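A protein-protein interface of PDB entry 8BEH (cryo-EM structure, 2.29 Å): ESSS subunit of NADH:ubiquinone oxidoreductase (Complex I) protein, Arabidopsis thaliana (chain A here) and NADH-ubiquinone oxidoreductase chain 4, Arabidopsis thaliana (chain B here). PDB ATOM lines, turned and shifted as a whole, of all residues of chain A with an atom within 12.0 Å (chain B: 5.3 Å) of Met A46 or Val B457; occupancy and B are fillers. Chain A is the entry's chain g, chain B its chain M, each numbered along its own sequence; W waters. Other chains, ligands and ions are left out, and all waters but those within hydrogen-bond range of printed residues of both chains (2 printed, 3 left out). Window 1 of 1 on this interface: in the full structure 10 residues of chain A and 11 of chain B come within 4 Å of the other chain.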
ATOM      1  N   PRO A  41       0.296 -29.803  -6.803  1.00  0.00           N
ATOM      2  CA  PRO A  41       0.473 -29.736  -8.256  1.00  0.00           C
ATOM      3  C   PRO A  41       1.642 -28.843  -8.652  1.00  0.00           C
ATOM      4  O   PRO A  41       2.168 -28.064  -7.854  1.00  0.00           O
ATOM      5  CB  PRO A  41      -0.857 -29.154  -8.745  1.00  0.00           C
ATOM      6  CG  PRO A  41      -1.830 -29.420  -7.644  1.00  0.00           C
ATOM      7  CD  PRO A  41      -1.031 -29.326  -6.384  1.00  0.00           C
ATOM      8  N   LYS A  42       2.019 -28.971  -9.930  1.00  0.00           N
ATOM      9  CA  LYS A  42       3.108 -28.127 -10.480  1.00  0.00           C
ATOM     10  C   LYS A  42       2.504 -26.791 -10.920  1.00  0.00           C
ATOM     11  O   LYS A  42       1.408 -26.803 -11.519  1.00  0.00           O
ATOM     12  CB  LYS A  42       3.830 -28.859 -11.619  1.00  0.00           C
ATOM     13  CG  LYS A  42       2.946 -29.433 -12.717  1.00  0.00           C
ATOM     14  CD  LYS A  42       3.703 -29.831 -13.966  1.00  0.00           C
ATOM     15  CE  LYS A  42       4.452 -31.141 -13.841  1.00  0.00           C
ATOM     16  NZ  LYS A  42       3.527 -32.298 -13.775  1.00  0.00           N
ATOM     17  N   GLY A  43       3.184 -25.686 -10.621  1.00  0.00           N
ATOM     18  CA  GLY A  43       2.700 -24.359 -10.933  1.00  0.00           C
ATOM     19  C   GLY A  43       1.707 -23.835  -9.912  1.00  0.00           C
ATOM     20  O   GLY A  43       1.349 -24.488  -8.933  1.00  0.00           O
ATOM     21  N   TYR A  44       1.253 -22.614 -10.159  1.00  0.00           N
ATOM     22  CA  TYR A  44       0.211 -21.990  -9.361  1.00  0.00           C
ATOM     23  C   TYR A  44      -0.857 -21.482 -10.306  1.00  0.00           C
ATOM     24  O   TYR A  44      -0.537 -20.880 -11.334  1.00  0.00           O
ATOM     25  CB  TYR A  44       0.765 -20.845  -8.512  1.00  0.00           C
ATOM     26  CG  TYR A  44       1.566 -21.341  -7.342  1.00  0.00           C
ATOM     27  CD1 TYR A  44       0.997 -22.177  -6.399  1.00  0.00           C
ATOM     28  CD2 TYR A  44       2.903 -20.998  -7.198  1.00  0.00           C
ATOM     29  CE1 TYR A  44       1.727 -22.651  -5.343  1.00  0.00           C
ATOM     30  CE2 TYR A  44       3.642 -21.465  -6.134  1.00  0.00           C
ATOM     31  CZ  TYR A  44       3.048 -22.291  -5.209  1.00  0.00           C
ATOM     32  OH  TYR A  44       3.774 -22.763  -4.142  1.00  0.00           O
ATOM     33  N   PHE A  45      -2.116 -21.731  -9.967  1.00  0.00           N
ATOM     34  CA  PHE A  45      -3.210 -21.299 -10.820  1.00  0.00           C
ATOM     35  C   PHE A  45      -3.175 -19.788 -11.005  1.00  0.00           C
ATOM     36  O   PHE A  45      -3.213 -19.033 -10.028  1.00  0.00           O
ATOM     37  CB  PHE A  45      -4.546 -21.735 -10.231  1.00  0.00           C
ATOM     38  CG  PHE A  45      -5.718 -21.330 -11.064  1.00  0.00           C
ATOM     39  CD1 PHE A  45      -6.741 -20.570 -10.526  1.00  0.00           C
ATOM     40  CD2 PHE A  45      -5.778 -21.679 -12.399  1.00  0.00           C
ATOM     41  CE1 PHE A  45      -7.814 -20.189 -11.300  1.00  0.00           C
ATOM     42  CE2 PHE A  45      -6.849 -21.298 -13.180  1.00  0.00           C
ATOM     43  CZ  PHE A  45      -7.869 -20.551 -12.630  1.00  0.00           C
ATOM     44  N   MET A  46      -3.099 -19.354 -12.262  1.00  0.00           N
ATOM     45  CA  MET A  46      -2.977 -17.946 -12.636  1.00  0.00           C
ATOM     46  C   MET A  46      -1.711 -17.296 -12.077  1.00  0.00           C
ATOM     47  O   MET A  46      -1.664 -16.078 -11.897  1.00  0.00           O
ATOM     48  CB  MET A  46      -4.238 -17.165 -12.240  1.00  0.00           C
ATOM     49  CG  MET A  46      -5.462 -17.641 -13.026  1.00  0.00           C
ATOM     50  SD  MET A  46      -7.090 -17.092 -12.483  1.00  0.00           S
ATOM     51  CE  MET A  46      -6.737 -16.534 -10.831  1.00  0.00           C
ATOM     52  N   ASN A  47      -0.685 -18.110 -11.816  1.00  0.00           N
ATOM     53  CA  ASN A  47       0.675 -17.650 -11.505  1.00  0.00           C
ATOM     54  C   ASN A  47       0.720 -16.695 -10.316  1.00  0.00           C
ATOM     55  O   ASN A  47       1.548 -15.786 -10.262  1.00  0.00           O
ATOM     56  CB  ASN A  47       1.337 -17.005 -12.728  1.00  0.00           C
ATOM     57  CG  ASN A  47       1.798 -18.020 -13.757  1.00  0.00           C
ATOM     58  OD1 ASN A  47       1.037 -18.901 -14.151  1.00  0.00           O
ATOM     59  ND2 ASN A  47       3.050 -17.913 -14.185  1.00  0.00           N
ATOM     60  N   ARG A  48      -0.160 -16.902  -9.345  1.00  0.00           N
ATOM     61  CA  ARG A  48      -0.126 -16.134  -8.107  1.00  0.00           C
ATOM     62  C   ARG A  48       0.377 -17.028  -6.983  1.00  0.00           C
ATOM     63  O   ARG A  48      -0.119 -18.141  -6.798  1.00  0.00           O
ATOM     64  CB  ARG A  48      -1.493 -15.547  -7.750  1.00  0.00           C
ATOM     65  CG  ARG A  48      -2.657 -16.509  -7.828  1.00  0.00           C
ATOM     66  CD  ARG A  48      -3.870 -15.946  -7.108  1.00  0.00           C
ATOM     67  NE  ARG A  48      -4.589 -14.944  -7.888  1.00  0.00           N
ATOM     68  CZ  ARG A  48      -5.902 -14.933  -8.058  1.00  0.00           C
ATOM     69  NH1 ARG A  48      -6.674 -15.875  -7.541  1.00  0.00           N
ATOM     70  NH2 ARG A  48      -6.453 -13.964  -8.779  1.00  0.00           N
ATOM     71  N   THR A  49       1.370 -16.547  -6.251  1.00  0.00           N
ATOM     72  CA  THR A  49       1.889 -17.311  -5.137  1.00  0.00           C
ATOM     73  C   THR A  49       0.844 -17.380  -4.024  1.00  0.00           C
ATOM     74  O   THR A  49       0.074 -16.441  -3.827  1.00  0.00           O
ATOM     75  CB  THR A  49       3.181 -16.698  -4.619  1.00  0.00           C
ATOM     76  OG1 THR A  49       2.950 -15.335  -4.242  1.00  0.00           O
ATOM     77  CG2 THR A  49       4.242 -16.743  -5.698  1.00  0.00           C
ATOM     78  N   PRO A  50       0.776 -18.502  -3.305  1.00  0.00           N
ATOM     79  CA  PRO A  50      -0.255 -18.650  -2.277  1.00  0.00           C
ATOM     80  C   PRO A  50      -0.033 -17.681  -1.131  1.00  0.00           C
ATOM     81  O   PRO A  50       1.092 -17.207  -0.908  1.00  0.00           O
ATOM     82  CB  PRO A  50      -0.059 -20.108  -1.840  1.00  0.00           C
ATOM     83  CG  PRO A  50       1.462 -20.015  -2.053  1.00  0.00           C
ATOM     84  CD  PRO A  50       1.390 -19.852  -3.446  1.00  0.00           C
ATOM     85  N   PRO A  51      -1.083 -17.326  -0.403  1.00  0.00           N
ATOM     86  CA  PRO A  51      -0.905 -16.459   0.767  1.00  0.00           C
ATOM     87  C   PRO A  51      -0.199 -17.209   1.886  1.00  0.00           C
ATOM     88  O   PRO A  51      -0.103 -18.437   1.893  1.00  0.00           O
ATOM     89  CB  PRO A  51      -2.334 -16.071   1.144  1.00  0.00           C
ATOM     90  CG  PRO A  51      -3.170 -17.178   0.616  1.00  0.00           C
ATOM     91  CD  PRO A  51      -2.493 -17.689  -0.615  1.00  0.00           C
ATOM     92  N   ARG A  57      -5.988 -14.553   0.464  1.00  0.00           N
ATOM     93  CA  ARG A  57      -5.521 -13.714  -0.628  1.00  0.00           C
ATOM     94  C   ARG A  57      -6.244 -12.372  -0.596  1.00  0.00           C
ATOM     95  O   ARG A  57      -7.444 -12.300  -0.330  1.00  0.00           O
ATOM     96  CB  ARG A  57      -5.738 -14.416  -1.969  1.00  0.00           C
ATOM     97  CG  ARG A  57      -5.437 -13.546  -3.170  1.00  0.00           C
ATOM     98  CD  ARG A  57      -5.784 -14.232  -4.473  1.00  0.00           C
ATOM     99  NE  ARG A  57      -7.222 -14.300  -4.688  1.00  0.00           N
ATOM    100  CZ  ARG A  57      -7.914 -13.425  -5.404  1.00  0.00           C
ATOM    101  NH1 ARG A  57      -7.341 -12.361  -5.936  1.00  0.00           N
ATOM    102  NH2 ARG A  57      -9.218 -13.617  -5.577  1.00  0.00           N
ATOM    103  N   LYS A  58      -5.493 -11.302  -0.828  1.00  0.00           N
ATOM    104  CA  LYS A  58      -6.070  -9.966  -0.873  1.00  0.00           C
ATOM    105  C   LYS A  58      -6.669  -9.749  -2.258  1.00  0.00           C
ATOM    106  O   LYS A  58      -6.000  -9.967  -3.271  1.00  0.00           O
ATOM    107  CB  LYS A  58      -4.986  -8.938  -0.521  1.00  0.00           C
ATOM    108  CG  LYS A  58      -5.354  -7.446  -0.429  1.00  0.00           C
ATOM    109  CD  LYS A  58      -4.240  -6.486  -0.030  1.00  0.00           C
ATOM    110  CE  LYS A  58      -4.717  -5.038   0.004  1.00  0.00           C
ATOM    111  NZ  LYS A  58      -3.636  -4.091   0.392  1.00  0.00           N
ATOM    112  N   TRP A  59      -7.941  -9.358  -2.301  1.00  0.00           N
ATOM    113  CA  TRP A  59      -8.629  -9.140  -3.570  1.00  0.00           C
ATOM    114  C   TRP A  59      -8.207  -7.816  -4.187  1.00  0.00           C
ATOM    115  O   TRP A  59      -8.188  -6.786  -3.511  1.00  0.00           O
ATOM    116  CB  TRP A  59     -10.145  -9.150  -3.375  1.00  0.00           C
ATOM    117  CG  TRP A  59     -10.757 -10.508  -3.323  1.00  0.00           C
ATOM    118  CD1 TRP A  59     -10.130 -11.682  -3.028  1.00  0.00           C
ATOM    119  CD2 TRP A  59     -12.130 -10.836  -3.563  1.00  0.00           C
ATOM    120  NE1 TRP A  59     -11.025 -12.721  -3.077  1.00  0.00           N
ATOM    121  CE2 TRP A  59     -12.261 -12.228  -3.399  1.00  0.00           C
ATOM    122  CE3 TRP A  59     -13.260 -10.087  -3.901  1.00  0.00           C
ATOM    123  CZ2 TRP A  59     -13.476 -12.888  -3.564  1.00  0.00           C
ATOM    124  CZ3 TRP A  59     -14.467 -10.743  -4.061  1.00  0.00           C
ATOM    125  CH2 TRP A  59     -14.564 -12.129  -3.896  1.00  0.00           C
ATOM    126  N   GLU A  60      -7.895  -7.837  -5.478  1.00  0.00           N
ATOM    127  CA  GLU A  60      -7.618  -6.586  -6.167  1.00  0.00           C
ATOM    128  C   GLU A  60      -8.895  -5.761  -6.304  1.00  0.00           C
ATOM    129  O   GLU A  60     -10.013  -6.272  -6.211  1.00  0.00           O
ATOM    130  CB  GLU A  60      -6.987  -6.845  -7.531  1.00  0.00           C
ATOM    131  CG  GLU A  60      -5.741  -7.705  -7.478  1.00  0.00           C
ATOM    132  CD  GLU A  60      -4.784  -7.426  -8.623  1.00  0.00           C
ATOM    133  OE1 GLU A  60      -5.213  -7.510  -9.791  1.00  0.00           O
ATOM    134  OE2 GLU A  60      -3.600  -7.132  -8.355  1.00  0.00           O
ATOM    135  N   TRP A  62     -10.498  -4.381  -8.671  1.00  0.00           N
ATOM    136  CA  TRP A  62     -11.455  -4.652  -9.736  1.00  0.00           C
ATOM    137  C   TRP A  62     -12.315  -5.883  -9.471  1.00  0.00           C
ATOM    138  O   TRP A  62     -13.354  -6.038 -10.116  1.00  0.00           O
ATOM    139  CB  TRP A  62     -10.718  -4.817 -11.070  1.00  0.00           C
ATOM    140  CG  TRP A  62      -9.728  -5.936 -11.049  1.00  0.00           C
ATOM    141  CD1 TRP A  62      -8.406  -5.850 -10.737  1.00  0.00           C
ATOM    142  CD2 TRP A  62      -9.982  -7.318 -11.332  1.00  0.00           C
ATOM    143  NE1 TRP A  62      -7.820  -7.085 -10.811  1.00  0.00           N
ATOM    144  CE2 TRP A  62      -8.764  -8.005 -11.175  1.00  0.00           C
ATOM    145  CE3 TRP A  62     -11.119  -8.039 -11.708  1.00  0.00           C
ATOM    146  CZ2 TRP A  62      -8.651  -9.377 -11.371  1.00  0.00           C
ATOM    147  CZ3 TRP A  62     -11.004  -9.400 -11.908  1.00  0.00           C
ATOM    148  CH2 TRP A  62      -9.779 -10.056 -11.739  1.00  0.00           C
ATOM    149  N   GLU A  63     -11.918  -6.744  -8.531  1.00  0.00           N
ATOM    150  CA  GLU A  63     -12.513  -8.076  -8.418  1.00  0.00           C
ATOM    151  C   GLU A  63     -13.983  -8.009  -8.022  1.00  0.00           C
ATOM    152  O   GLU A  63     -14.847  -8.551  -8.715  1.00  0.00           O
ATOM    153  CB  GLU A  63     -11.721  -8.913  -7.415  1.00  0.00           C
ATOM    154  CG  GLU A  63     -10.267  -9.122  -7.805  1.00  0.00           C
ATOM    155  CD  GLU A  63      -9.746 -10.499  -7.452  1.00  0.00           C
ATOM    156  OE1 GLU A  63     -10.473 -11.491  -7.644  1.00  0.00           O
ATOM    157  OE2 GLU A  63      -8.605 -10.580  -6.961  1.00  0.00           O
ATOM    158  N   CYS A  66     -16.433  -6.412 -10.649  1.00  0.00           N
ATOM    159  CA  CYS A  66     -16.582  -7.268 -11.819  1.00  0.00           C
ATOM    160  C   CYS A  66     -17.388  -8.518 -11.496  1.00  0.00           C
ATOM    161  O   CYS A  66     -18.230  -8.936 -12.294  1.00  0.00           O
ATOM    162  CB  CYS A  66     -15.210  -7.633 -12.381  1.00  0.00           C
ATOM    163  SG  CYS A  66     -14.463  -6.336 -13.396  1.00  0.00           S
ATOM    164  N   TYR A  67     -17.156  -9.121 -10.327  1.00  0.00           N
ATOM    165  CA  TYR A  67     -17.899 -10.323  -9.957  1.00  0.00           C
ATOM    166  C   TYR A  67     -19.371 -10.010  -9.716  1.00  0.00           C
ATOM    167  O   TYR A  67     -20.248 -10.791 -10.102  1.00  0.00           O
ATOM    168  CB  TYR A  67     -17.283 -10.978  -8.719  1.00  0.00           C
ATOM    169  CG  TYR A  67     -15.856 -11.439  -8.894  1.00  0.00           C
ATOM    170  CD1 TYR A  67     -15.339 -11.720 -10.154  1.00  0.00           C
ATOM    171  CD2 TYR A  67     -15.020 -11.577  -7.798  1.00  0.00           C
ATOM    172  CE1 TYR A  67     -14.033 -12.133 -10.311  1.00  0.00           C
ATOM    173  CE2 TYR A  67     -13.720 -11.989  -7.942  1.00  0.00           C
ATOM    174  CZ  TYR A  67     -13.227 -12.266  -9.196  1.00  0.00           C
ATOM    175  OH  TYR A  67     -11.924 -12.676  -9.331  1.00  0.00           O
ATOM    176  N   SER A  70     -20.924  -9.588 -13.029  1.00  0.00           N
ATOM    177  CA  SER A  70     -21.114 -10.878 -13.686  1.00  0.00           C
ATOM    178  C   SER A  70     -22.326 -11.612 -13.128  1.00  0.00           C
ATOM    179  O   SER A  70     -23.122 -12.183 -13.884  1.00  0.00           O
ATOM    180  CB  SER A  70     -19.859 -11.735 -13.529  1.00  0.00           C
ATOM    181  OG  SER A  70     -18.809 -11.250 -14.338  1.00  0.00           O
ATOM    182  N   ASN B 376      -2.292 -21.820 -20.482  1.00  0.00           N
ATOM    183  CA  ASN B 376      -3.616 -21.206 -20.396  1.00  0.00           C
ATOM    184  C   ASN B 376      -3.829 -20.208 -21.528  1.00  0.00           C
ATOM    185  O   ASN B 376      -4.864 -20.230 -22.215  1.00  0.00           O
ATOM    186  CB  ASN B 376      -3.791 -20.525 -19.039  1.00  0.00           C
ATOM    187  CG  ASN B 376      -4.079 -21.508 -17.929  1.00  0.00           C
ATOM    188  OD1 ASN B 376      -4.640 -22.574 -18.162  1.00  0.00           O
ATOM    189  ND2 ASN B 376      -3.693 -21.156 -16.715  1.00  0.00           N
ATOM    190  N   ILE B 380      -6.622 -20.509 -24.678  1.00  0.00           N
ATOM    191  CA  ILE B 380      -7.549 -19.425 -25.009  1.00  0.00           C
ATOM    192  C   ILE B 380      -7.278 -18.884 -26.414  1.00  0.00           C
ATOM    193  O   ILE B 380      -8.210 -18.630 -27.198  1.00  0.00           O
ATOM    194  CB  ILE B 380      -7.469 -18.326 -23.929  1.00  0.00           C
ATOM    195  CG1 ILE B 380      -8.038 -18.855 -22.607  1.00  0.00           C
ATOM    196  CG2 ILE B 380      -8.168 -17.050 -24.374  1.00  0.00           C
ATOM    197  CD1 ILE B 380      -7.836 -17.943 -21.424  1.00  0.00           C
ATOM    198  N   LEU B 452      -1.231 -16.160 -17.883  1.00  0.00           N
ATOM    199  CA  LEU B 452      -2.212 -15.130 -17.569  1.00  0.00           C
ATOM    200  C   LEU B 452      -2.431 -14.998 -16.067  1.00  0.00           C
ATOM    201  O   LEU B 452      -2.480 -15.992 -15.340  1.00  0.00           O
ATOM    202  CB  LEU B 452      -3.536 -15.436 -18.263  1.00  0.00           C
ATOM    203  CG  LEU B 452      -3.438 -15.920 -19.711  1.00  0.00           C
ATOM    204  CD1 LEU B 452      -4.730 -16.586 -20.128  1.00  0.00           C
ATOM    205  CD2 LEU B 452      -3.091 -14.769 -20.648  1.00  0.00           C
ATOM    206  N   ASN B 453      -2.561 -13.756 -15.604  1.00  0.00           N
ATOM    207  CA  ASN B 453      -2.972 -13.507 -14.234  1.00  0.00           C
ATOM    208  C   ASN B 453      -4.499 -13.534 -14.143  1.00  0.00           C
ATOM    209  O   ASN B 453      -5.202 -13.736 -15.136  1.00  0.00           O
ATOM    210  CB  ASN B 453      -2.410 -12.177 -13.720  1.00  0.00           C
ATOM    211  CG  ASN B 453      -2.669 -11.014 -14.659  1.00  0.00           C
ATOM    212  OD1 ASN B 453      -3.794 -10.783 -15.093  1.00  0.00           O
ATOM    213  ND2 ASN B 453      -1.626 -10.257 -14.953  1.00  0.00           N
ATOM    214  N   GLY B 454      -5.015 -13.309 -12.933  1.00  0.00           N
ATOM    215  CA  GLY B 454      -6.451 -13.391 -12.718  1.00  0.00           C
ATOM    216  C   GLY B 454      -7.239 -12.386 -13.537  1.00  0.00           C
ATOM    217  O   GLY B 454      -8.305 -12.707 -14.069  1.00  0.00           O
ATOM    218  N   ARG B 455      -6.719 -11.161 -13.659  1.00  0.00           N
ATOM    219  CA  ARG B 455      -7.414 -10.132 -14.428  1.00  0.00           C
ATOM    220  C   ARG B 455      -7.568 -10.539 -15.889  1.00  0.00           C
ATOM    221  O   ARG B 455      -8.639 -10.367 -16.478  1.00  0.00           O
ATOM    222  CB  ARG B 455      -6.673  -8.800 -14.314  1.00  0.00           C
ATOM    223  CG  ARG B 455      -7.507  -7.581 -14.694  1.00  0.00           C
ATOM    224  CD  ARG B 455      -6.779  -6.273 -14.395  1.00  0.00           C
ATOM    225  NE  ARG B 455      -5.335  -6.453 -14.425  1.00  0.00           N
ATOM    226  CZ  ARG B 455      -4.589  -6.374 -15.517  1.00  0.00           C
ATOM    227  NH1 ARG B 455      -5.109  -6.047 -16.687  1.00  0.00           N
ATOM    228  NH2 ARG B 455      -3.290  -6.642 -15.436  1.00  0.00           N
ATOM    229  N   GLU B 456      -6.507 -11.081 -16.484  1.00  0.00           N
ATOM    230  CA  GLU B 456      -6.551 -11.474 -17.889  1.00  0.00           C
ATOM    231  C   GLU B 456      -7.522 -12.630 -18.117  1.00  0.00           C
ATOM    232  O   GLU B 456      -8.292 -12.624 -19.089  1.00  0.00           O
ATOM    233  CB  GLU B 456      -5.136 -11.818 -18.358  1.00  0.00           C
ATOM    234  CG  GLU B 456      -4.272 -10.583 -18.624  1.00  0.00           C
ATOM    235  CD  GLU B 456      -2.776 -10.876 -18.658  1.00  0.00           C
ATOM    236  OE1 GLU B 456      -2.364 -12.006 -18.336  1.00  0.00           O
ATOM    237  OE2 GLU B 456      -2.010  -9.972 -19.034  1.00  0.00           O
ATOM    238  N   VAL B 457      -7.519 -13.615 -17.214  1.00  0.00           N
ATOM    239  CA  VAL B 457      -8.455 -14.731 -17.314  1.00  0.00           C
ATOM    240  C   VAL B 457      -9.890 -14.225 -17.227  1.00  0.00           C
ATOM    241  O   VAL B 457     -10.753 -14.593 -18.042  1.00  0.00           O
ATOM    242  CB  VAL B 457      -8.159 -15.778 -16.223  1.00  0.00           C
ATOM    243  CG1 VAL B 457      -9.326 -16.753 -16.077  1.00  0.00           C
ATOM    244  CG2 VAL B 457      -6.862 -16.514 -16.520  1.00  0.00           C
ATOM    245  N   PHE B 458     -10.163 -13.353 -16.250  1.00  0.00           N
ATOM    246  CA  PHE B 458     -11.508 -12.807 -16.130  1.00  0.00           C
ATOM    247  C   PHE B 458     -11.902 -12.037 -17.378  1.00  0.00           C
ATOM    248  O   PHE B 458     -13.045 -12.130 -17.831  1.00  0.00           O
ATOM    249  CB  PHE B 458     -11.649 -11.902 -14.911  1.00  0.00           C
ATOM    250  CG  PHE B 458     -12.994 -11.253 -14.832  1.00  0.00           C
ATOM    251  CD1 PHE B 458     -14.082 -11.955 -14.338  1.00  0.00           C
ATOM    252  CD2 PHE B 458     -13.193  -9.972 -15.320  1.00  0.00           C
ATOM    253  CE1 PHE B 458     -15.330 -11.379 -14.298  1.00  0.00           C
ATOM    254  CE2 PHE B 458     -14.437  -9.395 -15.287  1.00  0.00           C
ATOM    255  CZ  PHE B 458     -15.509 -10.096 -14.775  1.00  0.00           C
ATOM    256  N   ILE B 459     -10.977 -11.250 -17.932  1.00  0.00           N
ATOM    257  CA  ILE B 459     -11.273 -10.501 -19.148  1.00  0.00           C
ATOM    258  C   ILE B 459     -11.688 -11.451 -20.262  1.00  0.00           C
ATOM    259  O   ILE B 459     -12.640 -11.185 -21.002  1.00  0.00           O
ATOM    260  CB  ILE B 459     -10.061  -9.636 -19.550  1.00  0.00           C
ATOM    261  CG1 ILE B 459     -10.020  -8.345 -18.722  1.00  0.00           C
ATOM    262  CG2 ILE B 459     -10.081  -9.322 -21.033  1.00  0.00           C
ATOM    263  CD1 ILE B 459      -8.719  -7.581 -18.836  1.00  0.00           C
ATOM    264  N   PHE B 460     -11.001 -12.588 -20.380  1.00  0.00           N
ATOM    265  CA  PHE B 460     -11.322 -13.508 -21.466  1.00  0.00           C
ATOM    266  C   PHE B 460     -12.651 -14.232 -21.250  1.00  0.00           C
ATOM    267  O   PHE B 460     -13.322 -14.570 -22.230  1.00  0.00           O
ATOM    268  CB  PHE B 460     -10.187 -14.506 -21.665  1.00  0.00           C
ATOM    269  CG  PHE B 460      -9.053 -13.960 -22.476  1.00  0.00           C
ATOM    270  CD1 PHE B 460      -9.263 -13.521 -23.771  1.00  0.00           C
ATOM    271  CD2 PHE B 460      -7.786 -13.849 -21.933  1.00  0.00           C
ATOM    272  CE1 PHE B 460      -8.225 -13.006 -24.517  1.00  0.00           C
ATOM    273  CE2 PHE B 460      -6.747 -13.334 -22.673  1.00  0.00           C
ATOM    274  CZ  PHE B 460      -6.966 -12.908 -23.967  1.00  0.00           C
ATOM    275  N   ILE B 461     -13.063 -14.457 -19.995  1.00  0.00           N
ATOM    276  CA  ILE B 461     -14.242 -15.300 -19.745  1.00  0.00           C
ATOM    277  C   ILE B 461     -15.498 -14.840 -20.495  1.00  0.00           C
ATOM    278  O   ILE B 461     -16.116 -15.668 -21.179  1.00  0.00           O
ATOM    279  CB  ILE B 461     -14.482 -15.447 -18.234  1.00  0.00           C
ATOM    280  CG1 ILE B 461     -13.377 -16.273 -17.586  1.00  0.00           C
ATOM    281  CG2 ILE B 461     -15.838 -16.096 -17.971  1.00  0.00           C
ATOM    282  CD1 ILE B 461     -13.314 -16.121 -16.087  1.00  0.00           C
HETATM  283  O   HOH W   1      -4.609 -10.060 -11.757  1.00  0.00           O
HETATM  284  O   HOH W   2      -4.062  -6.770 -12.048  1.00  0.00           O
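Met A46 touches Leu B452. Asn B453 touches Met A46. CE of Met A46 touches CA of Gly B454, 3.7 Å away. Met A46 touches Val B457. Gly B454 touches Arg A48 (CA to NH2, 3.98 Å). Trp A62 touches Gly B454 (CH2 to O, 3.8 Å). CA of Arg B455 touches CZ2 of Trp A62, at 3.4 Å. Trp A62 touches Phe B458. CZ of Phe B458 touches CB of Cys A66, at 3.4 Å. OG of Ser A70 touches CE1 of Phe B458, at 3.5 Å.
Water W2 bridges the side-chain carboxylate (OE1) of Glu A60 (2.6 Å) and the guanidinium group (NE) of Arg B455 (2.7 Å). Water W1 lies within hydrogen-bond range of N of Arg B455 (3.0 Å), OE1 of Glu A60 (3.3 Å) and N of Gly B454 (3.5 Å).
Met A46 touches just these residues of chain B: Leu B452, Asn B453, Gly B454 and Val B457. Of chain A, only Met A46 (3.9 Å) comes within 4 Å of Val B457. Leu B452 touches just one residue of chain A: Met A46 (3.4 Å). Printed residues of chain A within 4 Å of Asn B453: Met A46. No residue of chain A comes within 4 Å of Glu B456. No residue of chain A comes within 4 Å of Ile B459. No residue of chain A comes within 4 Å of Phe B460. No residue of chain A comes within 4 Å of Ile B461. Of the printed residues of chain A, Arg B455 touches Trp A62. Of the printed residues of chain A, Gly B454 touches Met A46, Arg A48 and Trp A62. Printed residues of chain B within 4 Å of Arg A48: Gly B454 (3.98 Å). Of the printed residues of chain B, Ser A70 touches Phe B458. Printed residues of chain B within 4 Å of Trp A62: Gly B454 (3.8 Å), Arg B455 (3.4 Å) and Phe B458 (3.96 Å). The nearest residue of chain B that does not touch Met A46 is Asn B376 (4.8 Å). The nearest residue of chain A that does not touch Val B457 is Phe A45 (5.3 Å). The nearest printed residue of chain B that does not touch Arg A48 is Arg B455 (5.6 Å).
Of the 12 printed residues of chain B, 6 touch a printed residue of chain A. Hydrophobic or aromatic side chains of chain B that line the printed part of chain A: Val B457 and Phe B458. Printed residues of chain A that touch a printed residue of chain B: Met A46, Arg A48, Trp A62, Cys A66 and Ser A70. Hydrophobic or aromatic side chains of chain A within 4 Å of the printed part of chain B: Met A46 and Trp A62. Among the printed residues, 10 pairs touch across the chains.
The side-chain amide oxygen of Asn B453 lies within hydrogen-bond range of the backbone NH of Arg B455 (3.3 Å). The side-chain amide oxygen (OD1) of Asn B453 sits at hydrogen-bond distance from the backbone NH (N) of Glu B456 (3.1 Å). OE1 of Glu A60 sits at hydrogen-bond distance from NE1 of Trp A62 (2.8 Å). The backbone carbonyl oxygen (O) of Trp A62 sits close to the side-chain sulfur (SG) of Cys A66. The backbone carbonyl oxygen (O) of Cys A66 sits at hydrogen-bond distance from the side-chain hydroxyl (OG) of Ser A70, at 3.1 Å.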
